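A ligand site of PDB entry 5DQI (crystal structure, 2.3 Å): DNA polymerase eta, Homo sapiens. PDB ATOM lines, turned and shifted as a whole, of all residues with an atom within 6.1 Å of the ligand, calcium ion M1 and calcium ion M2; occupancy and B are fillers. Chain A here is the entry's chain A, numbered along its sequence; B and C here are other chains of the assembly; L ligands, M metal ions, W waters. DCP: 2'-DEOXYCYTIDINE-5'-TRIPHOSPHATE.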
ATOM      1  N   ASP A  16      -8.308  -2.358   6.801  1.00  0.00           N
ATOM      2  CA  ASP A  16      -7.727  -3.259   5.859  1.00  0.00           C
ATOM      3  C   ASP A  16      -6.908  -2.477   4.837  1.00  0.00           C
ATOM      4  O   ASP A  16      -7.400  -1.513   4.231  1.00  0.00           O
ATOM      5  CB  ASP A  16      -8.817  -4.029   5.167  1.00  0.00           C
ATOM      6  CG  ASP A  16      -8.356  -4.639   3.859  1.00  0.00           C
ATOM      7  OD1 ASP A  16      -7.895  -5.795   3.850  1.00  0.00           O
ATOM      8  OD2 ASP A  16      -8.435  -3.957   2.814  1.00  0.00           O
ATOM      9  N   MET A  17      -5.669  -2.909   4.582  1.00  0.00           N
ATOM     10  CA  MET A  17      -4.763  -2.125   3.742  1.00  0.00           C
ATOM     11  C   MET A  17      -5.170  -2.224   2.290  1.00  0.00           C
ATOM     12  O   MET A  17      -5.617  -3.303   1.789  1.00  0.00           O
ATOM     13  CB  MET A  17      -3.334  -2.634   3.881  1.00  0.00           C
ATOM     14  CG  MET A  17      -2.852  -2.856   5.298  1.00  0.00           C
ATOM     15  SD  MET A  17      -3.094  -1.420   6.321  1.00  0.00           S
ATOM     16  CE  MET A  17      -2.136  -0.271   5.403  1.00  0.00           C
ATOM     17  N   ASP A  18      -5.042  -1.106   1.598  1.00  0.00           N
ATOM     18  CA  ASP A  18      -5.311  -1.075   0.183  1.00  0.00           C
ATOM     19  C   ASP A  18      -4.245  -1.862  -0.588  1.00  0.00           C
ATOM     20  O   ASP A  18      -3.054  -1.613  -0.409  1.00  0.00           O
ATOM     21  CB  ASP A  18      -5.380   0.360  -0.313  1.00  0.00           C
ATOM     22  CG  ASP A  18      -6.400   1.190   0.415  1.00  0.00           C
ATOM     23  OD1 ASP A  18      -7.404   0.631   0.896  1.00  0.00           O
ATOM     24  OD2 ASP A  18      -6.183   2.404   0.532  1.00  0.00           O
ATOM     25  N   CYS A  19      -4.692  -2.823  -1.419  1.00  0.00           N
ATOM     26  CA  CYS A  19      -3.799  -3.600  -2.278  1.00  0.00           C
ATOM     27  C   CYS A  19      -2.419  -3.826  -1.605  1.00  0.00           C
ATOM     28  O   CYS A  19      -1.397  -3.361  -2.090  1.00  0.00           O
ATOM     29  CB  CYS A  19      -3.677  -2.946  -3.684  1.00  0.00           C
ATOM     30  SG  CYS A  19      -3.020  -1.222  -3.790  1.00  0.00           S
ATOM     31  N   PHE A  20      -2.407  -4.571  -0.510  1.00  0.00           N
ATOM     32  CA  PHE A  20      -1.329  -4.510   0.447  1.00  0.00           C
ATOM     33  C   PHE A  20       0.050  -4.886  -0.097  1.00  0.00           C
ATOM     34  O   PHE A  20       0.986  -4.098   0.012  1.00  0.00           O
ATOM     35  CB  PHE A  20      -1.625  -5.393   1.637  1.00  0.00           C
ATOM     36  CG  PHE A  20      -0.647  -5.225   2.767  1.00  0.00           C
ATOM     37  CD1 PHE A  20      -0.246  -3.965   3.164  1.00  0.00           C
ATOM     38  CD2 PHE A  20      -0.133  -6.315   3.427  1.00  0.00           C
ATOM     39  CE1 PHE A  20       0.656  -3.778   4.184  1.00  0.00           C
ATOM     40  CE2 PHE A  20       0.749  -6.146   4.517  1.00  0.00           C
ATOM     41  CZ  PHE A  20       1.150  -4.869   4.873  1.00  0.00           C
ATOM     42  N   PHE A  21       0.160  -6.083  -0.689  1.00  0.00           N
ATOM     43  CA  PHE A  21       1.467  -6.535  -1.194  1.00  0.00           C
ATOM     44  C   PHE A  21       1.984  -5.558  -2.218  1.00  0.00           C
ATOM     45  O   PHE A  21       3.156  -5.226  -2.183  1.00  0.00           O
ATOM     46  CB  PHE A  21       1.419  -7.931  -1.771  1.00  0.00           C
ATOM     47  CG  PHE A  21       1.310  -9.011  -0.751  1.00  0.00           C
ATOM     48  CD1 PHE A  21       0.898  -8.764   0.536  1.00  0.00           C
ATOM     49  CD2 PHE A  21       1.577 -10.327  -1.123  1.00  0.00           C
ATOM     50  CE1 PHE A  21       0.772  -9.793   1.460  1.00  0.00           C
ATOM     51  CE2 PHE A  21       1.458 -11.363  -0.202  1.00  0.00           C
ATOM     52  CZ  PHE A  21       1.050 -11.090   1.097  1.00  0.00           C
ATOM     53  N   VAL A  22       1.115  -5.083  -3.100  1.00  0.00           N
ATOM     54  CA  VAL A  22       1.509  -4.032  -4.053  1.00  0.00           C
ATOM     55  C   VAL A  22       2.112  -2.818  -3.316  1.00  0.00           C
ATOM     56  O   VAL A  22       3.217  -2.420  -3.624  1.00  0.00           O
ATOM     57  CB  VAL A  22       0.336  -3.561  -4.924  1.00  0.00           C
ATOM     58  CG1 VAL A  22       0.732  -2.333  -5.700  1.00  0.00           C
ATOM     59  CG2 VAL A  22      -0.098  -4.633  -5.898  1.00  0.00           C
ATOM     60  N   GLN A  41       3.785 -14.397  -8.282  1.00  0.00           N
ATOM     61  CA  GLN A  41       4.368 -15.565  -7.589  1.00  0.00           C
ATOM     62  C   GLN A  41       4.813 -16.605  -8.646  1.00  0.00           C
ATOM     63  O   GLN A  41       3.988 -17.020  -9.450  1.00  0.00           O
ATOM     64  CB  GLN A  41       3.262 -16.170  -6.694  1.00  0.00           C
ATOM     65  CG  GLN A  41       3.714 -16.830  -5.385  1.00  0.00           C
ATOM     66  CD  GLN A  41       2.535 -17.260  -4.500  1.00  0.00           C
ATOM     67  OE1 GLN A  41       1.566 -17.862  -4.973  1.00  0.00           O
ATOM     68  NE2 GLN A  41       2.623 -16.959  -3.203  1.00  0.00           N
ATOM     69  N   ILE A  51      -1.051 -12.159  -7.349  1.00  0.00           N
ATOM     70  CA  ILE A  51      -1.710 -12.249  -6.029  1.00  0.00           C
ATOM     71  C   ILE A  51      -2.170 -10.918  -5.418  1.00  0.00           C
ATOM     72  O   ILE A  51      -2.875 -10.919  -4.381  1.00  0.00           O
ATOM     73  CB  ILE A  51      -0.821 -12.999  -4.999  1.00  0.00           C
ATOM     74  CG1 ILE A  51       0.549 -12.331  -4.863  1.00  0.00           C
ATOM     75  CG2 ILE A  51      -0.677 -14.479  -5.365  1.00  0.00           C
ATOM     76  CD1 ILE A  51       1.345 -12.908  -3.710  1.00  0.00           C
ATOM     77  N   ALA A  52      -1.767  -9.795  -6.015  1.00  0.00           N
ATOM     78  CA  ALA A  52      -2.219  -8.493  -5.590  1.00  0.00           C
ATOM     79  C   ALA A  52      -2.064  -7.527  -6.743  1.00  0.00           C
ATOM     80  O   ALA A  52      -1.164  -7.683  -7.555  1.00  0.00           O
ATOM     81  CB  ALA A  52      -1.436  -8.023  -4.362  1.00  0.00           C
ATOM     82  N   VAL A  53      -2.975  -6.571  -6.819  1.00  0.00           N
ATOM     83  CA  VAL A  53      -3.183  -5.750  -8.007  1.00  0.00           C
ATOM     84  C   VAL A  53      -3.423  -4.313  -7.570  1.00  0.00           C
ATOM     85  O   VAL A  53      -4.294  -4.067  -6.749  1.00  0.00           O
ATOM     86  CB  VAL A  53      -4.412  -6.224  -8.844  1.00  0.00           C
ATOM     87  CG1 VAL A  53      -4.467  -5.514 -10.183  1.00  0.00           C
ATOM     88  CG2 VAL A  53      -4.391  -7.700  -9.070  1.00  0.00           C
ATOM     89  N   TYR A  55      -4.796  -0.510  -8.004  1.00  0.00           N
ATOM     90  CA  TYR A  55      -6.086  -0.059  -8.527  1.00  0.00           C
ATOM     91  C   TYR A  55      -6.001   0.465  -9.964  1.00  0.00           C
ATOM     92  O   TYR A  55      -6.922   0.288 -10.743  1.00  0.00           O
ATOM     93  CB  TYR A  55      -6.719   0.967  -7.597  1.00  0.00           C
ATOM     94  CG  TYR A  55      -7.305   0.282  -6.350  1.00  0.00           C
ATOM     95  CD1 TYR A  55      -8.669  -0.025  -6.272  1.00  0.00           C
ATOM     96  CD2 TYR A  55      -6.487  -0.104  -5.281  1.00  0.00           C
ATOM     97  CE1 TYR A  55      -9.204  -0.648  -5.143  1.00  0.00           C
ATOM     98  CE2 TYR A  55      -7.017  -0.705  -4.162  1.00  0.00           C
ATOM     99  CZ  TYR A  55      -8.366  -0.985  -4.087  1.00  0.00           C
ATOM    100  OH  TYR A  55      -8.871  -1.609  -2.958  1.00  0.00           O
ATOM    101  N   ARG A  58      -6.311  -2.550 -12.012  1.00  0.00           N
ATOM    102  CA  ARG A  58      -7.684  -3.059 -11.897  1.00  0.00           C
ATOM    103  C   ARG A  58      -8.621  -2.426 -12.943  1.00  0.00           C
ATOM    104  O   ARG A  58      -9.475  -3.121 -13.487  1.00  0.00           O
ATOM    105  CB  ARG A  58      -8.266  -2.797 -10.496  1.00  0.00           C
ATOM    106  CG  ARG A  58      -7.722  -3.701  -9.412  1.00  0.00           C
ATOM    107  CD  ARG A  58      -8.300  -3.422  -8.042  1.00  0.00           C
ATOM    108  NE  ARG A  58      -7.387  -3.903  -7.016  1.00  0.00           N
ATOM    109  CZ  ARG A  58      -7.683  -4.104  -5.739  1.00  0.00           C
ATOM    110  NH1 ARG A  58      -8.887  -3.878  -5.239  1.00  0.00           N
ATOM    111  NH2 ARG A  58      -6.718  -4.536  -4.928  1.00  0.00           N
ATOM    112  N   ARG A  64      -6.466 -10.763  -9.276  1.00  0.00           N
ATOM    113  CA  ARG A  64      -5.856 -11.883  -8.578  1.00  0.00           C
ATOM    114  C   ARG A  64      -6.116 -13.218  -9.309  1.00  0.00           C
ATOM    115  O   ARG A  64      -7.052 -13.314 -10.117  1.00  0.00           O
ATOM    116  CB  ARG A  64      -6.385 -11.918  -7.149  1.00  0.00           C
ATOM    117  CG  ARG A  64      -5.780 -13.001  -6.275  1.00  0.00           C
ATOM    118  CD  ARG A  64      -5.495 -12.536  -4.861  1.00  0.00           C
ATOM    119  NE  ARG A  64      -6.662 -11.932  -4.231  1.00  0.00           N
ATOM    120  CZ  ARG A  64      -6.639 -10.808  -3.512  1.00  0.00           C
ATOM    121  NH1 ARG A  64      -5.519 -10.116  -3.318  1.00  0.00           N
ATOM    122  NH2 ARG A  64      -7.777 -10.367  -2.994  1.00  0.00           N
ATOM    123  N   SER A 116      -6.189 -10.915   9.458  1.00  0.00           N
ATOM    124  CA  SER A 116      -5.309 -11.458   8.435  1.00  0.00           C
ATOM    125  C   SER A 116      -3.994 -10.733   8.414  1.00  0.00           C
ATOM    126  O   SER A 116      -3.720  -9.877   9.274  1.00  0.00           O
ATOM    127  CB  SER A 116      -5.996 -11.430   7.029  1.00  0.00           C
ATOM    128  OG  SER A 116      -6.032 -10.107   6.468  1.00  0.00           O
ATOM    129  N   ILE A 117      -3.169 -11.025   7.403  1.00  0.00           N
ATOM    130  CA  ILE A 117      -1.887 -10.359   7.251  1.00  0.00           C
ATOM    131  C   ILE A 117      -2.107  -8.881   7.046  1.00  0.00           C
ATOM    132  O   ILE A 117      -1.213  -8.078   7.267  1.00  0.00           O
ATOM    133  CB  ILE A 117      -1.077 -10.938   6.099  1.00  0.00           C
ATOM    134  CG1 ILE A 117       0.415 -10.620   6.339  1.00  0.00           C
ATOM    135  CG2 ILE A 117      -1.595 -10.436   4.766  1.00  0.00           C
ATOM    136  CD1 ILE A 117       1.360 -11.010   5.212  1.00  0.00           C
ATOM    137  N   ASP A 118      -3.333  -8.553   6.690  1.00  0.00           N
ATOM    138  CA  ASP A 118      -3.694  -7.290   6.067  1.00  0.00           C
ATOM    139  C   ASP A 118      -4.709  -6.441   6.827  1.00  0.00           C
ATOM    140  O   ASP A 118      -4.909  -5.296   6.498  1.00  0.00           O
ATOM    141  CB  ASP A 118      -4.371  -7.665   4.726  1.00  0.00           C
ATOM    142  CG  ASP A 118      -4.506  -6.531   3.840  1.00  0.00           C
ATOM    143  OD1 ASP A 118      -3.662  -5.666   3.936  1.00  0.00           O
ATOM    144  OD2 ASP A 118      -5.440  -6.473   3.068  1.00  0.00           O
ATOM    145  N   GLU A 119      -5.441  -7.044   7.761  1.00  0.00           N
ATOM    146  CA  GLU A 119      -6.544  -6.378   8.375  1.00  0.00           C
ATOM    147  C   GLU A 119      -6.698  -6.841   9.822  1.00  0.00           C
ATOM    148  O   GLU A 119      -6.216  -7.895  10.220  1.00  0.00           O
ATOM    149  CB  GLU A 119      -7.834  -6.630   7.580  1.00  0.00           C
ATOM    150  CG  GLU A 119      -8.310  -8.047   7.621  1.00  0.00           C
ATOM    151  CD  GLU A 119      -9.387  -8.316   6.601  1.00  0.00           C
ATOM    152  OE1 GLU A 119     -10.555  -8.539   6.991  1.00  0.00           O
ATOM    153  OE2 GLU A 119      -9.078  -8.286   5.398  1.00  0.00           O
ATOM    154  N   LYS A 227     -16.794  -4.851   8.549  1.00  0.00           N
ATOM    155  CA  LYS A 227     -16.101  -5.437   7.406  1.00  0.00           C
ATOM    156  C   LYS A 227     -16.791  -5.075   6.087  1.00  0.00           C
ATOM    157  O   LYS A 227     -16.151  -4.664   5.125  1.00  0.00           O
ATOM    158  CB  LYS A 227     -16.005  -6.956   7.586  1.00  0.00           C
ATOM    159  CG  LYS A 227     -15.472  -7.757   6.394  1.00  0.00           C
ATOM    160  CD  LYS A 227     -13.968  -7.624   6.260  1.00  0.00           C
ATOM    161  CE  LYS A 227     -13.407  -8.458   5.108  1.00  0.00           C
ATOM    162  NZ  LYS A 227     -12.011  -8.102   4.736  1.00  0.00           N
ATOM    163  N   LYS A 234     -13.509   2.168  -1.211  1.00  0.00           N
ATOM    164  CA  LYS A 234     -12.149   1.741  -1.253  1.00  0.00           C
ATOM    165  C   LYS A 234     -11.633   2.326  -2.538  1.00  0.00           C
ATOM    166  O   LYS A 234     -12.341   2.316  -3.514  1.00  0.00           O
ATOM    167  CB  LYS A 234     -12.030   0.207  -1.263  1.00  0.00           C
ATOM    168  CG  LYS A 234     -11.489  -0.412  -0.002  1.00  0.00           C
ATOM    169  CD  LYS A 234     -10.851  -1.776  -0.317  1.00  0.00           C
ATOM    170  CE  LYS A 234      -9.954  -2.300   0.817  1.00  0.00           C
ATOM    171  NZ  LYS A 234      -8.633  -1.612   1.004  1.00  0.00           N
ATOM    172  N   PRO A 235     -10.387   2.786  -2.560  1.00  0.00           N
ATOM    173  CA  PRO A 235      -9.380   2.816  -1.506  1.00  0.00           C
ATOM    174  C   PRO A 235      -9.249   4.132  -0.796  1.00  0.00           C
ATOM    175  O   PRO A 235      -9.909   5.116  -1.159  1.00  0.00           O
ATOM    176  CB  PRO A 235      -8.085   2.512  -2.269  1.00  0.00           C
ATOM    177  CG  PRO A 235      -8.308   3.078  -3.647  1.00  0.00           C
ATOM    178  CD  PRO A 235      -9.779   2.952  -3.908  1.00  0.00           C
ATOM    179  P    DA B   8     -12.735 -11.747   2.890  1.00  0.00           P
ATOM    180  OP1  DA B   8     -13.659 -11.722   4.048  1.00  0.00           O
ATOM    181  OP2  DA B   8     -12.941 -10.884   1.704  1.00  0.00           O
ATOM    182  O5'  DA B   8     -11.328 -11.476   3.549  1.00  0.00           O
ATOM    183  C5'  DA B   8     -10.581 -12.623   4.025  1.00  0.00           C
ATOM    184  C4'  DA B   8      -9.450 -13.048   3.106  1.00  0.00           C
ATOM    185  O4'  DA B   8      -9.554 -14.360   2.514  1.00  0.00           O
ATOM    186  C3'  DA B   8      -9.098 -12.133   1.921  1.00  0.00           C
ATOM    187  O3'  DA B   8      -7.981 -11.338   2.265  1.00  0.00           O
ATOM    188  C2'  DA B   8      -8.658 -13.092   0.821  1.00  0.00           C
ATOM    189  C1'  DA B   8      -8.496 -14.389   1.585  1.00  0.00           C
ATOM    190  N9   DA B   8      -8.564 -15.649   0.837  1.00  0.00           N
ATOM    191  C8   DA B   8      -9.646 -16.172   0.166  1.00  0.00           C
ATOM    192  N7   DA B   8      -9.392 -17.314  -0.429  1.00  0.00           N
ATOM    193  C5   DA B   8      -8.060 -17.560  -0.124  1.00  0.00           C
ATOM    194  C6   DA B   8      -7.193 -18.615  -0.479  1.00  0.00           C
ATOM    195  N6   DA B   8      -7.558 -19.666  -1.219  1.00  0.00           N
ATOM    196  N1   DA B   8      -5.919 -18.564  -0.007  1.00  0.00           N
ATOM    197  C2   DA B   8      -5.554 -17.513   0.733  1.00  0.00           C
ATOM    198  N3   DA B   8      -6.274 -16.455   1.122  1.00  0.00           N
ATOM    199  C4   DA B   8      -7.539 -16.542   0.655  1.00  0.00           C
ATOM    200  P    DC B   9      -7.188 -11.427   3.638  1.00  0.00           P
ATOM    201  OP1  DC B   9      -7.925 -12.078   4.750  1.00  0.00           O
ATOM    202  OP2  DC B   9      -6.671 -10.055   3.866  1.00  0.00           O
ATOM    203  O5'  DC B   9      -6.019 -12.470   3.348  1.00  0.00           O
ATOM    204  C5'  DC B   9      -4.696 -11.944   3.050  1.00  0.00           C
ATOM    205  C4'  DC B   9      -3.615 -12.969   3.250  1.00  0.00           C
ATOM    206  O4'  DC B   9      -3.516 -13.281   4.654  1.00  0.00           O
ATOM    207  C3'  DC B   9      -3.850 -14.299   2.522  1.00  0.00           C
ATOM    208  O3'  DC B   9      -2.658 -14.779   1.906  1.00  0.00           O
ATOM    209  C2'  DC B   9      -4.284 -15.238   3.627  1.00  0.00           C
ATOM    210  C1'  DC B   9      -3.550 -14.693   4.838  1.00  0.00           C
ATOM    211  N1   DC B   9      -4.188 -14.973   6.132  1.00  0.00           N
ATOM    212  C2   DC B   9      -3.470 -14.700   7.300  1.00  0.00           C
ATOM    213  O2   DC B   9      -2.339 -14.214   7.204  1.00  0.00           O
ATOM    214  N3   DC B   9      -4.042 -14.942   8.501  1.00  0.00           N
ATOM    215  C4   DC B   9      -5.263 -15.477   8.559  1.00  0.00           C
ATOM    216  N4   DC B   9      -5.778 -15.716   9.772  1.00  0.00           N
ATOM    217  C5   DC B   9      -6.000 -15.805   7.382  1.00  0.00           C
ATOM    218  C6   DC B   9      -5.440 -15.529   6.210  1.00  0.00           C
ATOM    219  P    DT C   3      -5.517 -23.171 -12.864  1.00  0.00           P
ATOM    220  OP1  DT C   3      -6.352 -24.263 -13.443  1.00  0.00           O
ATOM    221  OP2  DT C   3      -5.745 -21.775 -13.297  1.00  0.00           O
ATOM    222  O5'  DT C   3      -5.660 -23.241 -11.276  1.00  0.00           O
ATOM    223  C5'  DT C   3      -5.623 -22.053 -10.482  1.00  0.00           C
ATOM    224  C4'  DT C   3      -4.179 -21.701 -10.190  1.00  0.00           C
ATOM    225  O4'  DT C   3      -4.081 -20.307  -9.812  1.00  0.00           O
ATOM    226  C3'  DT C   3      -3.552 -22.500  -9.051  1.00  0.00           C
ATOM    227  O3'  DT C   3      -2.260 -22.990  -9.426  1.00  0.00           O
ATOM    228  C2'  DT C   3      -3.401 -21.479  -7.940  1.00  0.00           C
ATOM    229  C1'  DT C   3      -3.123 -20.246  -8.770  1.00  0.00           C
ATOM    230  N1   DT C   3      -3.298 -18.975  -8.052  1.00  0.00           N
ATOM    231  C2   DT C   3      -2.243 -18.091  -7.997  1.00  0.00           C
ATOM    232  O2   DT C   3      -1.159 -18.302  -8.517  1.00  0.00           O
ATOM    233  N3   DT C   3      -2.503 -16.943  -7.293  1.00  0.00           N
ATOM    234  C4   DT C   3      -3.683 -16.601  -6.652  1.00  0.00           C
ATOM    235  O4   DT C   3      -3.764 -15.534  -6.051  1.00  0.00           O
ATOM    236  C5   DT C   3      -4.740 -17.581  -6.747  1.00  0.00           C
ATOM    237  C7   DT C   3      -6.057 -17.297  -6.085  1.00  0.00           C
ATOM    238  C6   DT C   3      -4.502 -18.702  -7.430  1.00  0.00           C
ATOM    239  P    DG C   4      -1.473 -23.991  -8.471  1.00  0.00           P
ATOM    240  OP1  DG C   4      -0.425 -24.681  -9.280  1.00  0.00           O
ATOM    241  OP2  DG C   4      -2.468 -24.797  -7.730  1.00  0.00           O
ATOM    242  O5'  DG C   4      -0.811 -23.026  -7.396  1.00  0.00           O
ATOM    243  C5'  DG C   4       0.181 -22.056  -7.758  1.00  0.00           C
ATOM    244  C4'  DG C   4       0.868 -21.516  -6.531  1.00  0.00           C
ATOM    245  O4'  DG C   4       0.054 -20.468  -5.940  1.00  0.00           O
ATOM    246  C3'  DG C   4       1.088 -22.530  -5.419  1.00  0.00           C
ATOM    247  O3'  DG C   4       2.279 -22.126  -4.767  1.00  0.00           O
ATOM    248  C2'  DG C   4      -0.120 -22.327  -4.526  1.00  0.00           C
ATOM    249  C1'  DG C   4      -0.280 -20.819  -4.610  1.00  0.00           C
ATOM    250  N9   DG C   4      -1.625 -20.318  -4.343  1.00  0.00           N
ATOM    251  C8   DG C   4      -2.817 -20.902  -4.683  1.00  0.00           C
ATOM    252  N7   DG C   4      -3.855 -20.199  -4.333  1.00  0.00           N
ATOM    253  C5   DG C   4      -3.315 -19.061  -3.742  1.00  0.00           C
ATOM    254  C6   DG C   4      -3.947 -17.930  -3.175  1.00  0.00           C
ATOM    255  O6   DG C   4      -5.158 -17.701  -3.077  1.00  0.00           O
ATOM    256  N1   DG C   4      -3.029 -17.021  -2.686  1.00  0.00           N
ATOM    257  C2   DG C   4      -1.663 -17.177  -2.735  1.00  0.00           C
ATOM    258  N2   DG C   4      -0.931 -16.182  -2.204  1.00  0.00           N
ATOM    259  N3   DG C   4      -1.056 -18.226  -3.254  1.00  0.00           N
ATOM    260  C4   DG C   4      -1.933 -19.131  -3.735  1.00  0.00           C
ATOM    261  C1  5EJ C   5      -5.668 -22.343  -1.145  1.00  0.00           C
ATOM    262  C2  5EJ C   5      -2.091 -19.367  -0.146  1.00  0.00           C
ATOM    263  P   5EJ C   5       2.744 -22.947  -3.403  1.00  0.00           P
ATOM    264  OP1 5EJ C   5       4.238 -22.990  -3.465  1.00  0.00           O
ATOM    265  O5' 5EJ C   5       2.234 -22.055  -2.220  1.00  0.00           O
ATOM    266  C5' 5EJ C   5       2.856 -20.762  -2.154  1.00  0.00           C
ATOM    267  C4' 5EJ C   5       2.460 -20.010  -0.887  1.00  0.00           C
ATOM    268  C3' 5EJ C   5       2.514 -20.955   0.280  1.00  0.00           C
ATOM    269  O3' 5EJ C   5       3.220 -20.243   1.293  1.00  0.00           O
ATOM    270  C2' 5EJ C   5       1.067 -21.261   0.590  1.00  0.00           C
ATOM    271  C1' 5EJ C   5       0.338 -20.021   0.094  1.00  0.00           C
ATOM    272  O4' 5EJ C   5       1.114 -19.557  -1.018  1.00  0.00           O
ATOM    273  N1  5EJ C   5      -1.023 -20.319  -0.328  1.00  0.00           N
ATOM    274  C6  5EJ C   5      -1.257 -21.514  -0.873  1.00  0.00           C
ATOM    275  C5  5EJ C   5      -2.529 -21.883  -1.270  1.00  0.00           C
ATOM    276  C7  5EJ C   5      -2.674 -23.271  -1.865  1.00  0.00           C
ATOM    277  C4  5EJ C   5      -3.641 -20.899  -1.091  1.00  0.00           C
ATOM    278  N3  5EJ C   5      -3.357 -19.686  -0.551  1.00  0.00           N
ATOM    279  O2  5EJ C   5      -1.877 -18.224   0.348  1.00  0.00           O
ATOM    280  O4  5EJ C   5      -4.938 -21.128  -1.444  1.00  0.00           O
ATOM    281  OP2 5EJ C   5       2.139 -24.300  -3.353  1.00  0.00           O
ATOM    282  C3  5EJ C   5      -6.228 -22.929  -2.432  1.00  0.00           C
HETATM  283  N1  DCP L   1      -3.372 -12.412  -0.615  1.00  0.00           N
HETATM  284  C2  DCP L   1      -2.922 -13.574  -1.291  1.00  0.00           C
HETATM  285  N3  DCP L   1      -3.852 -14.474  -1.796  1.00  0.00           N
HETATM  286  C4  DCP L   1      -5.217 -14.241  -1.729  1.00  0.00           C
HETATM  287  C5  DCP L   1      -5.646 -13.070  -1.101  1.00  0.00           C
HETATM  288  C6  DCP L   1      -4.714 -12.144  -0.552  1.00  0.00           C
HETATM  289  O2  DCP L   1      -1.693 -13.790  -1.383  1.00  0.00           O
HETATM  290  N4  DCP L   1      -6.133 -15.119  -2.258  1.00  0.00           N
HETATM  291  C1' DCP L   1      -2.398 -11.460  -0.077  1.00  0.00           C
HETATM  292  C2' DCP L   1      -2.183 -10.438  -1.171  1.00  0.00           C
HETATM  293  C3' DCP L   1      -3.019  -9.266  -0.698  1.00  0.00           C
HETATM  294  C4' DCP L   1      -3.090  -9.347   0.799  1.00  0.00           C
HETATM  295  O4' DCP L   1      -2.907 -10.751   1.087  1.00  0.00           O
HETATM  296  O3' DCP L   1      -2.449  -8.030  -1.045  1.00  0.00           O
HETATM  297  C5' DCP L   1      -4.402  -8.797   1.325  1.00  0.00           C
HETATM  298  O5' DCP L   1      -5.508  -9.449   0.683  1.00  0.00           O
HETATM  299  PA  DCP L   1      -6.843  -8.647   0.358  1.00  0.00           P
HETATM  300  O1A DCP L   1      -7.862  -9.701  -0.024  1.00  0.00           O
HETATM  301  O2A DCP L   1      -7.195  -7.605   1.404  1.00  0.00           O
HETATM  302  O3A DCP L   1      -6.608  -7.785  -0.982  1.00  0.00           O
HETATM  303  PB  DCP L   1      -5.626  -6.539  -1.228  1.00  0.00           P
HETATM  304  O1B DCP L   1      -4.570  -7.047  -2.203  1.00  0.00           O
HETATM  305  O2B DCP L   1      -5.119  -5.943   0.057  1.00  0.00           O
HETATM  306  O3B DCP L   1      -6.549  -5.531  -2.082  1.00  0.00           O
HETATM  307  PG  DCP L   1      -7.841  -4.766  -1.499  1.00  0.00           P
HETATM  308  O1G DCP L   1      -8.914  -5.245  -2.466  1.00  0.00           O
HETATM  309  O2G DCP L   1      -8.067  -5.310  -0.141  1.00  0.00           O
HETATM  310  O3G DCP L   1      -7.468  -3.269  -1.581  1.00  0.00           O
HETATM  311 CA    CA M   1      -6.723  -5.363   1.637  1.00  0.00          CA
HETATM  312 CA    CA M   2      -7.755  -7.967   3.621  1.00  0.00          CA
HETATM  313  O   HOH W   1      -4.724  -6.883  -4.699  1.00  0.00           O
HETATM  314  O   HOH W   2     -10.248  -6.644   0.817  1.00  0.00           O
HETATM  315  O   HOH W   3      -9.685  -8.519   2.406  1.00  0.00           O
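OH of Tyr 55 sits at hydrogen-bond distance from O3G of the ligand, 2.6 Å away. O6 of DG 4 of chain C lies within hydrogen-bond range of a nitrogen (N4) of the ligand, at 2.9 Å. The backbone NH of Cys 19 is in hydrogen-bond range of an oxygen (O3G) of the ligand. O1A of the ligand sits close to O3' of DA 8 of chain B (2.8 Å). The guanidinium group of Arg 58 lies within salt-bridge range of an oxygen (O1G) of the ligand, at 3.1 Å. An oxygen (O1A) of the ligand is in salt-bridge range of the guanidinium group (NH2) of Arg 64, 3.0 Å away. An oxygen (O2B) of the ligand sits close to the backbone NH (N) of Phe 20 (3.1 Å). N of Phe 21 is in hydrogen-bond range of O3' of the ligand (3.3 Å). The side-chain amino group (NZ) of Lys 234 is in salt-bridge range of an oxygen (O3G) of the ligand (3.3 Å).
The backbone NH (N) of Asp 118 lies close to the side-chain hydroxyl (OG) of Ser 116, 3.1 Å away. The backbone NH of Glu 119 lies close to the side-chain hydroxyl of Ser 116 (3.4 Å). OE1 of Glu 119 is in salt-bridge range of NZ of Lys 227. N of Ile 117 lies within hydrogen-bond range of O2 of DC 9 of chain B, at 3.3 Å. The side-chain hydroxyl of Tyr 55 sits close to the guanidinium group of Arg 58, at 3.2 Å. N3 of DG 4 of chain C lies close to the side-chain amide oxygen (OE1) of Gln 41 (3.2 Å). The backbone carbonyl oxygen of Val 53 lies within hydrogen-bond range of the guanidinium group of Arg 58, at 3.1 Å. The side-chain carboxylate (OD1) of Asp 18 lies within salt-bridge range of the side-chain amino group (NZ) of Lys 234.
Residues that only touch the ligand: Ile 51, Ala 52, Asp 18 and Ile 117. Of the 26 residues printed, 17 come within 4 Å of the ligand. The nearest printed residue that does not touch the ligand is DT 3 of chain C (4.4 Å).
Within 4 Å of calcium ion M1: Asp 16, Met 17 and Asp 118.
Ser 116 touches calcium ion M2. O3' of DA 8 of chain B touches calcium ion M2, 3.6 Å away. Of the 26 residues printed, 6 come within 4 Å of calcium ion M2.
Calcium ion M1 is bound by OD2 of Asp 118 (2.2 Å), O2G of the ligand (2.2 Å), O2A of the ligand (2.3 Å), O2B of the ligand (2.3 Å), O of Met 17 (2.3 Å), OD2 of Asp 16 (2.5 Å) and OD1 of Asp 16 (2.5 Å).
Calcium ion M2 is bound by OD1 of Asp 16. Calcium ion M2 is bound by OE2 of Glu 119, 2.2 Å away. O2A of the ligand binds calcium ion M2, 2.3 Å away. Calcium ion M2 is bound by water W3, 2.3 Å away. OP2 of DC 9 of chain B is bound to calcium ion M2. The side-chain carboxylate (OD2) of Asp 118 binds calcium ion M2, 2.8 Å away.
Water W3 lies within hydrogen-bond range of an oxygen (O1A) of the ligand (3.3 Å), O3' of DA 8 of chain B (3.3 Å) and the side-chain amino group (NZ) of Lys 227 (3.3 Å). Water W1 lies within hydrogen-bond range of an oxygen (O1B) of the ligand (2.5 Å), the backbone NH of Val 53 (2.8 Å) and the guanidinium group of Arg 58 (3.1 Å).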
